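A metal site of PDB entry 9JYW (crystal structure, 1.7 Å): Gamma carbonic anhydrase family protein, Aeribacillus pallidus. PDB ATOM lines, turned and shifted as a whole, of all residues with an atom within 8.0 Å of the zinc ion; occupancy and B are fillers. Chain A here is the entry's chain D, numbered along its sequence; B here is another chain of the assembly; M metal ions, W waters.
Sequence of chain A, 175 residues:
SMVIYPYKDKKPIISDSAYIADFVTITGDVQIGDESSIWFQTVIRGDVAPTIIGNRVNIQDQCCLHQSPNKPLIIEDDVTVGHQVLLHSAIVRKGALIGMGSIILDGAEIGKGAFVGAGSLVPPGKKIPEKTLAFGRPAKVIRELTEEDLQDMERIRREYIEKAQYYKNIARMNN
A ring nitrogen (NE2) of His 66 is in hydrogen-bond range of the guanidinium group (NH1) of Arg 45 (3.4 Å). The side-chain carboxylate (OD1) of Asp 47 sits at hydrogen-bond distance from a ring nitrogen (NE2) of His 66 (2.7 Å). N of His 66 lies within hydrogen-bond range of O of Leu 87 (3.0 Å). The backbone carbonyl oxygen (O) of His 66 lies within hydrogen-bond range of the backbone NH (N) of Ser 89 (3.0 Å). The backbone NH (N) of His 83 of chain B lies within hydrogen-bond range of the side-chain amide oxygen (OE1) of Gln 60 of chain B, 3.2 Å away. A ring nitrogen (ND1) of His 83 of chain B sits at hydrogen-bond distance from the side-chain carboxylate (OD1) of Asp 61 of chain B, at 2.8 Å. The side-chain sulfur (SG) of Cys 64 is in hydrogen-bond range of a ring nitrogen (ND1) of His 83 of chain B (3.5 Å). A ring nitrogen (ND1) of His 88 lies within hydrogen-bond range of the side-chain carboxylate (OD2) of Asp 106 (2.6 Å).
The zinc ion is bound by a ring nitrogen (ND1) of His 66 (2.1 Å), a ring nitrogen (NE2) of His 83 of chain B (2.1 Å), a ring nitrogen (NE2) of His 88 (2.2 Å) and water W1 (2.3 Å).
The nearest printed residue that does not touch the zinc ion is Tyr 160 of chain B (4.1 Å).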
ATOM      1  N   ARG A  45       0.341  23.054   7.965  1.00  0.00           N
ATOM      2  CA  ARG A  45      -0.306  21.741   7.740  1.00  0.00           C
ATOM      3  C   ARG A  45      -0.080  21.357   6.291  1.00  0.00           C
ATOM      4  O   ARG A  45      -0.646  21.992   5.410  1.00  0.00           O
ATOM      5  CB  ARG A  45      -1.791  21.742   8.110  1.00  0.00           C
ATOM      6  CG  ARG A  45      -2.048  21.542   9.590  1.00  0.00           C
ATOM      7  CD  ARG A  45      -3.458  21.050   9.842  1.00  0.00           C
ATOM      8  NE  ARG A  45      -4.503  22.000   9.574  1.00  0.00           N
ATOM      9  CZ  ARG A  45      -5.466  21.903   8.659  1.00  0.00           C
ATOM     10  NH1 ARG A  45      -5.555  20.845   7.858  1.00  0.00           N
ATOM     11  NH2 ARG A  45      -6.377  22.861   8.539  1.00  0.00           N
ATOM     12  N   ASP A  47      -1.089  18.841   4.326  1.00  0.00           N
ATOM     13  CA  ASP A  47      -2.015  17.687   4.189  1.00  0.00           C
ATOM     14  C   ASP A  47      -2.907  17.840   2.963  1.00  0.00           C
ATOM     15  O   ASP A  47      -3.811  16.976   2.808  1.00  0.00           O
ATOM     16  CB  ASP A  47      -2.780  17.446   5.485  1.00  0.00           C
ATOM     17  CG  ASP A  47      -3.544  18.662   6.014  1.00  0.00           C
ATOM     18  OD1 ASP A  47      -3.887  19.555   5.210  1.00  0.00           O
ATOM     19  OD2 ASP A  47      -3.772  18.703   7.230  1.00  0.00           O
ATOM     20  N   VAL A  48      -2.720  18.866   2.112  1.00  0.00           N
ATOM     21  CA  VAL A  48      -3.537  19.026   0.875  1.00  0.00           C
ATOM     22  C   VAL A  48      -2.628  19.009  -0.363  1.00  0.00           C
ATOM     23  O   VAL A  48      -2.985  18.345  -1.368  1.00  0.00           O
ATOM     24  CB  VAL A  48      -4.438  20.270   0.953  1.00  0.00           C
ATOM     25  CG1 VAL A  48      -5.139  20.551  -0.364  1.00  0.00           C
ATOM     26  CG2 VAL A  48      -5.446  20.149   2.094  1.00  0.00           C
ATOM     27  N   CYS A  64      -0.300  31.058   9.508  1.00  0.00           N
ATOM     28  CA  CYS A  64      -1.015  29.842   9.110  1.00  0.00           C
ATOM     29  C   CYS A  64      -0.682  29.575   7.643  1.00  0.00           C
ATOM     30  O   CYS A  64      -0.940  30.457   6.835  1.00  0.00           O
ATOM     31  CB  CYS A  64      -2.520  29.996   9.302  1.00  0.00           C
ATOM     32  SG  CYS A  64      -3.366  28.448   8.909  1.00  0.00           S
ATOM     33  N   LEU A  65      -0.040  28.455   7.369  1.00  0.00           N
ATOM     34  CA  LEU A  65       0.340  28.021   6.006  1.00  0.00           C
ATOM     35  C   LEU A  65      -0.459  26.773   5.660  1.00  0.00           C
ATOM     36  O   LEU A  65      -0.401  25.778   6.421  1.00  0.00           O
ATOM     37  CB  LEU A  65       1.838  27.729   5.989  1.00  0.00           C
ATOM     38  CG  LEU A  65       2.752  28.936   5.739  1.00  0.00           C
ATOM     39  CD1 LEU A  65       2.581  30.012   6.817  1.00  0.00           C
ATOM     40  CD2 LEU A  65       4.205  28.477   5.706  1.00  0.00           C
ATOM     41  N   HIS A  66      -1.232  26.841   4.574  1.00  0.00           N
ATOM     42  CA  HIS A  66      -2.076  25.699   4.142  1.00  0.00           C
ATOM     43  C   HIS A  66      -2.180  25.722   2.626  1.00  0.00           C
ATOM     44  O   HIS A  66      -1.549  26.580   1.983  1.00  0.00           O
ATOM     45  CB  HIS A  66      -3.432  25.691   4.871  1.00  0.00           C
ATOM     46  CG  HIS A  66      -4.066  24.346   4.885  1.00  0.00           C
ATOM     47  ND1 HIS A  66      -5.350  24.157   4.583  1.00  0.00           N
ATOM     48  CD2 HIS A  66      -3.549  23.107   5.084  1.00  0.00           C
ATOM     49  CE1 HIS A  66      -5.692  22.891   4.623  1.00  0.00           C
ATOM     50  NE2 HIS A  66      -4.592  22.194   4.915  1.00  0.00           N
ATOM     51  N   GLN A  67      -2.860  24.731   2.056  1.00  0.00           N
ATOM     52  CA  GLN A  67      -3.002  24.630   0.589  1.00  0.00           C
ATOM     53  C   GLN A  67      -4.449  24.274   0.228  1.00  0.00           C
ATOM     54  O   GLN A  67      -5.116  23.615   1.056  1.00  0.00           O
ATOM     55  CB  GLN A  67      -2.069  23.576  -0.022  1.00  0.00           C
ATOM     56  CG  GLN A  67      -0.704  23.484   0.631  1.00  0.00           C
ATOM     57  CD  GLN A  67      -0.732  22.684   1.919  1.00  0.00           C
ATOM     58  OE1 GLN A  67      -1.444  21.694   2.062  1.00  0.00           O
ATOM     59  NE2 GLN A  67       0.048  23.135   2.893  1.00  0.00           N
ATOM     60  N   SER A  68      -4.810  24.567  -1.013  1.00  0.00           N
ATOM     61  CA  SER A  68      -5.994  23.995  -1.719  1.00  0.00           C
ATOM     62  C   SER A  68      -5.471  22.944  -2.705  1.00  0.00           C
ATOM     63  O   SER A  68      -4.277  22.922  -3.030  1.00  0.00           O
ATOM     64  CB  SER A  68      -6.818  25.064  -2.350  1.00  0.00           C
ATOM     65  OG  SER A  68      -6.066  25.790  -3.312  1.00  0.00           O
ATOM     66  N   LEU A  86      -1.545  34.826   6.731  1.00  0.00           N
ATOM     67  CA  LEU A  86      -2.164  33.612   6.199  1.00  0.00           C
ATOM     68  C   LEU A  86      -1.670  33.426   4.766  1.00  0.00           C
ATOM     69  O   LEU A  86      -1.854  34.370   3.964  1.00  0.00           O
ATOM     70  CB  LEU A  86      -3.684  33.837   6.280  1.00  0.00           C
ATOM     71  CG  LEU A  86      -4.601  32.740   5.745  1.00  0.00           C
ATOM     72  CD1 LEU A  86      -4.237  31.355   6.240  1.00  0.00           C
ATOM     73  CD2 LEU A  86      -6.037  33.084   6.105  1.00  0.00           C
ATOM     74  N   LEU A  87      -0.995  32.322   4.494  1.00  0.00           N
ATOM     75  CA  LEU A  87      -0.583  31.916   3.132  1.00  0.00           C
ATOM     76  C   LEU A  87      -1.378  30.671   2.755  1.00  0.00           C
ATOM     77  O   LEU A  87      -1.283  29.671   3.488  1.00  0.00           O
ATOM     78  CB  LEU A  87       0.915  31.622   3.059  1.00  0.00           C
ATOM     79  CG  LEU A  87       1.847  32.738   3.489  1.00  0.00           C
ATOM     80  CD1 LEU A  87       3.303  32.256   3.448  1.00  0.00           C
ATOM     81  CD2 LEU A  87       1.660  33.967   2.637  1.00  0.00           C
ATOM     82  N   HIS A  88      -2.136  30.719   1.666  1.00  0.00           N
ATOM     83  CA  HIS A  88      -2.955  29.576   1.235  1.00  0.00           C
ATOM     84  C   HIS A  88      -2.603  29.296  -0.211  1.00  0.00           C
ATOM     85  O   HIS A  88      -3.051  30.045  -1.060  1.00  0.00           O
ATOM     86  CB  HIS A  88      -4.439  29.871   1.479  1.00  0.00           C
ATOM     87  CG  HIS A  88      -5.224  28.641   1.800  1.00  0.00           C
ATOM     88  ND1 HIS A  88      -5.778  27.853   0.805  1.00  0.00           N
ATOM     89  CD2 HIS A  88      -5.524  28.020   2.957  1.00  0.00           C
ATOM     90  CE1 HIS A  88      -6.337  26.787   1.357  1.00  0.00           C
ATOM     91  NE2 HIS A  88      -6.214  26.921   2.603  1.00  0.00           N
ATOM     92  N   SER A  89      -1.747  28.313  -0.489  1.00  0.00           N
ATOM     93  CA  SER A  89      -1.299  27.958  -1.861  1.00  0.00           C
ATOM     94  C   SER A  89      -0.702  29.194  -2.533  1.00  0.00           C
ATOM     95  O   SER A  89      -0.878  29.393  -3.747  1.00  0.00           O
ATOM     96  CB  SER A  89      -2.435  27.351  -2.653  1.00  0.00           C
ATOM     97  OG  SER A  89      -2.692  26.026  -2.226  1.00  0.00           O
ATOM     98  N   ASP A 106      -5.075  31.634  -2.949  1.00  0.00           N
ATOM     99  CA  ASP A 106      -4.682  30.442  -3.749  1.00  0.00           C
ATOM    100  C   ASP A 106      -4.186  30.855  -5.140  1.00  0.00           C
ATOM    101  O   ASP A 106      -4.902  31.527  -5.883  1.00  0.00           O
ATOM    102  CB  ASP A 106      -5.828  29.434  -3.757  1.00  0.00           C
ATOM    103  CG  ASP A 106      -6.179  29.107  -2.320  1.00  0.00           C
ATOM    104  OD1 ASP A 106      -6.864  29.975  -1.667  1.00  0.00           O
ATOM    105  OD2 ASP A 106      -5.694  28.092  -1.815  1.00  0.00           O
ATOM    106  N   GLN B  60     -11.277  25.746  11.900  1.00  0.00           N
ATOM    107  CA  GLN B  60      -9.897  25.556  11.411  1.00  0.00           C
ATOM    108  C   GLN B  60      -8.898  26.262  12.340  1.00  0.00           C
ATOM    109  O   GLN B  60      -9.270  26.720  13.440  1.00  0.00           O
ATOM    110  CB  GLN B  60      -9.812  25.940   9.936  1.00  0.00           C
ATOM    111  CG  GLN B  60     -10.558  24.940   9.061  1.00  0.00           C
ATOM    112  CD  GLN B  60     -10.642  25.430   7.642  1.00  0.00           C
ATOM    113  OE1 GLN B  60      -9.798  26.212   7.192  1.00  0.00           O
ATOM    114  NE2 GLN B  60     -11.677  24.983   6.947  1.00  0.00           N
ATOM    115  N   ASP B  61      -7.635  26.232  11.970  1.00  0.00           N
ATOM    116  CA  ASP B  61      -6.504  26.611  12.847  1.00  0.00           C
ATOM    117  C   ASP B  61      -6.589  28.088  13.243  1.00  0.00           C
ATOM    118  O   ASP B  61      -6.957  28.927  12.422  1.00  0.00           O
ATOM    119  CB  ASP B  61      -5.190  26.282  12.143  1.00  0.00           C
ATOM    120  CG  ASP B  61      -5.255  25.026  11.283  1.00  0.00           C
ATOM    121  OD1 ASP B  61      -5.906  25.084  10.198  1.00  0.00           O
ATOM    122  OD2 ASP B  61      -4.747  23.983  11.735  1.00  0.00           O
ATOM    123  N   GLY B  82     -13.146  28.876   8.447  1.00  0.00           N
ATOM    124  CA  GLY B  82     -11.790  28.965   7.865  1.00  0.00           C
ATOM    125  C   GLY B  82     -10.717  29.346   8.859  1.00  0.00           C
ATOM    126  O   GLY B  82     -10.998  29.825   9.954  1.00  0.00           O
ATOM    127  N   HIS B  83      -9.463  29.140   8.468  1.00  0.00           N
ATOM    128  CA  HIS B  83      -8.287  29.504   9.290  1.00  0.00           C
ATOM    129  C   HIS B  83      -8.397  30.944   9.788  1.00  0.00           C
ATOM    130  O   HIS B  83      -8.758  31.821   9.000  1.00  0.00           O
ATOM    131  CB  HIS B  83      -6.982  29.432   8.513  1.00  0.00           C
ATOM    132  CG  HIS B  83      -6.844  28.215   7.654  1.00  0.00           C
ATOM    133  ND1 HIS B  83      -6.510  26.988   8.198  1.00  0.00           N
ATOM    134  CD2 HIS B  83      -6.982  28.022   6.318  1.00  0.00           C
ATOM    135  CE1 HIS B  83      -6.441  26.104   7.199  1.00  0.00           C
ATOM    136  NE2 HIS B  83      -6.729  26.747   6.113  1.00  0.00           N
ATOM    137  N   MET B 100     -11.597  31.964   5.408  1.00  0.00           N
ATOM    138  CA  MET B 100     -10.391  32.176   6.214  1.00  0.00           C
ATOM    139  C   MET B 100     -10.089  33.689   6.351  1.00  0.00           C
ATOM    140  O   MET B 100     -10.280  34.457   5.375  1.00  0.00           O
ATOM    141  CB  MET B 100      -9.225  31.400   5.583  1.00  0.00           C
ATOM    142  CG  MET B 100      -8.849  31.909   4.217  1.00  0.00           C
ATOM    143  SD  MET B 100      -7.603  30.842   3.408  1.00  0.00           S
ATOM    144  CE  MET B 100      -8.665  29.687   2.559  1.00  0.00           C
ATOM    145  N   ILE B 156     -15.328  20.161   1.029  1.00  0.00           N
ATOM    146  CA  ILE B 156     -14.461  20.659   2.138  1.00  0.00           C
ATOM    147  C   ILE B 156     -14.960  20.084   3.465  1.00  0.00           C
ATOM    148  O   ILE B 156     -14.132  19.599   4.242  1.00  0.00           O
ATOM    149  CB  ILE B 156     -14.422  22.203   2.175  1.00  0.00           C
ATOM    150  CG1 ILE B 156     -13.728  22.764   0.927  1.00  0.00           C
ATOM    151  CG2 ILE B 156     -13.762  22.696   3.455  1.00  0.00           C
ATOM    152  CD1 ILE B 156     -13.924  24.259   0.763  1.00  0.00           C
ATOM    153  N   GLU B 159     -14.104  16.297   3.607  1.00  0.00           N
ATOM    154  CA  GLU B 159     -12.634  16.144   3.685  1.00  0.00           C
ATOM    155  C   GLU B 159     -12.176  16.422   5.125  1.00  0.00           C
ATOM    156  O   GLU B 159     -11.309  15.693   5.633  1.00  0.00           O
ATOM    157  CB  GLU B 159     -11.947  17.041   2.656  1.00  0.00           C
ATOM    158  CG  GLU B 159     -10.472  17.320   2.894  1.00  0.00           C
ATOM    159  CD  GLU B 159     -10.041  18.745   2.548  1.00  0.00           C
ATOM    160  OE1 GLU B 159      -8.875  19.110   2.791  1.00  0.00           O
ATOM    161  OE2 GLU B 159     -10.900  19.505   2.039  1.00  0.00           O
ATOM    162  N   TYR B 160     -12.749  17.422   5.795  1.00  0.00           N
ATOM    163  CA  TYR B 160     -12.305  17.775   7.178  1.00  0.00           C
ATOM    164  C   TYR B 160     -12.724  16.670   8.161  1.00  0.00           C
ATOM    165  O   TYR B 160     -11.957  16.379   9.090  1.00  0.00           O
ATOM    166  CB  TYR B 160     -12.814  19.161   7.565  1.00  0.00           C
ATOM    167  CG  TYR B 160     -11.736  20.205   7.350  1.00  0.00           C
ATOM    168  CD1 TYR B 160     -10.739  20.383   8.296  1.00  0.00           C
ATOM    169  CD2 TYR B 160     -11.705  20.959   6.201  1.00  0.00           C
ATOM    170  CE1 TYR B 160      -9.730  21.331   8.125  1.00  0.00           C
ATOM    171  CE2 TYR B 160     -10.708  21.917   6.014  1.00  0.00           C
ATOM    172  CZ  TYR B 160      -9.719  22.096   6.977  1.00  0.00           C
ATOM    173  OH  TYR B 160      -8.713  23.013   6.798  1.00  0.00           O
HETATM  174 ZN    ZN M   1      -6.784  25.658   4.261  1.00  0.00          ZN
HETATM  175  O   HOH W   1      -8.812  24.589   4.022  1.00  0.00           O
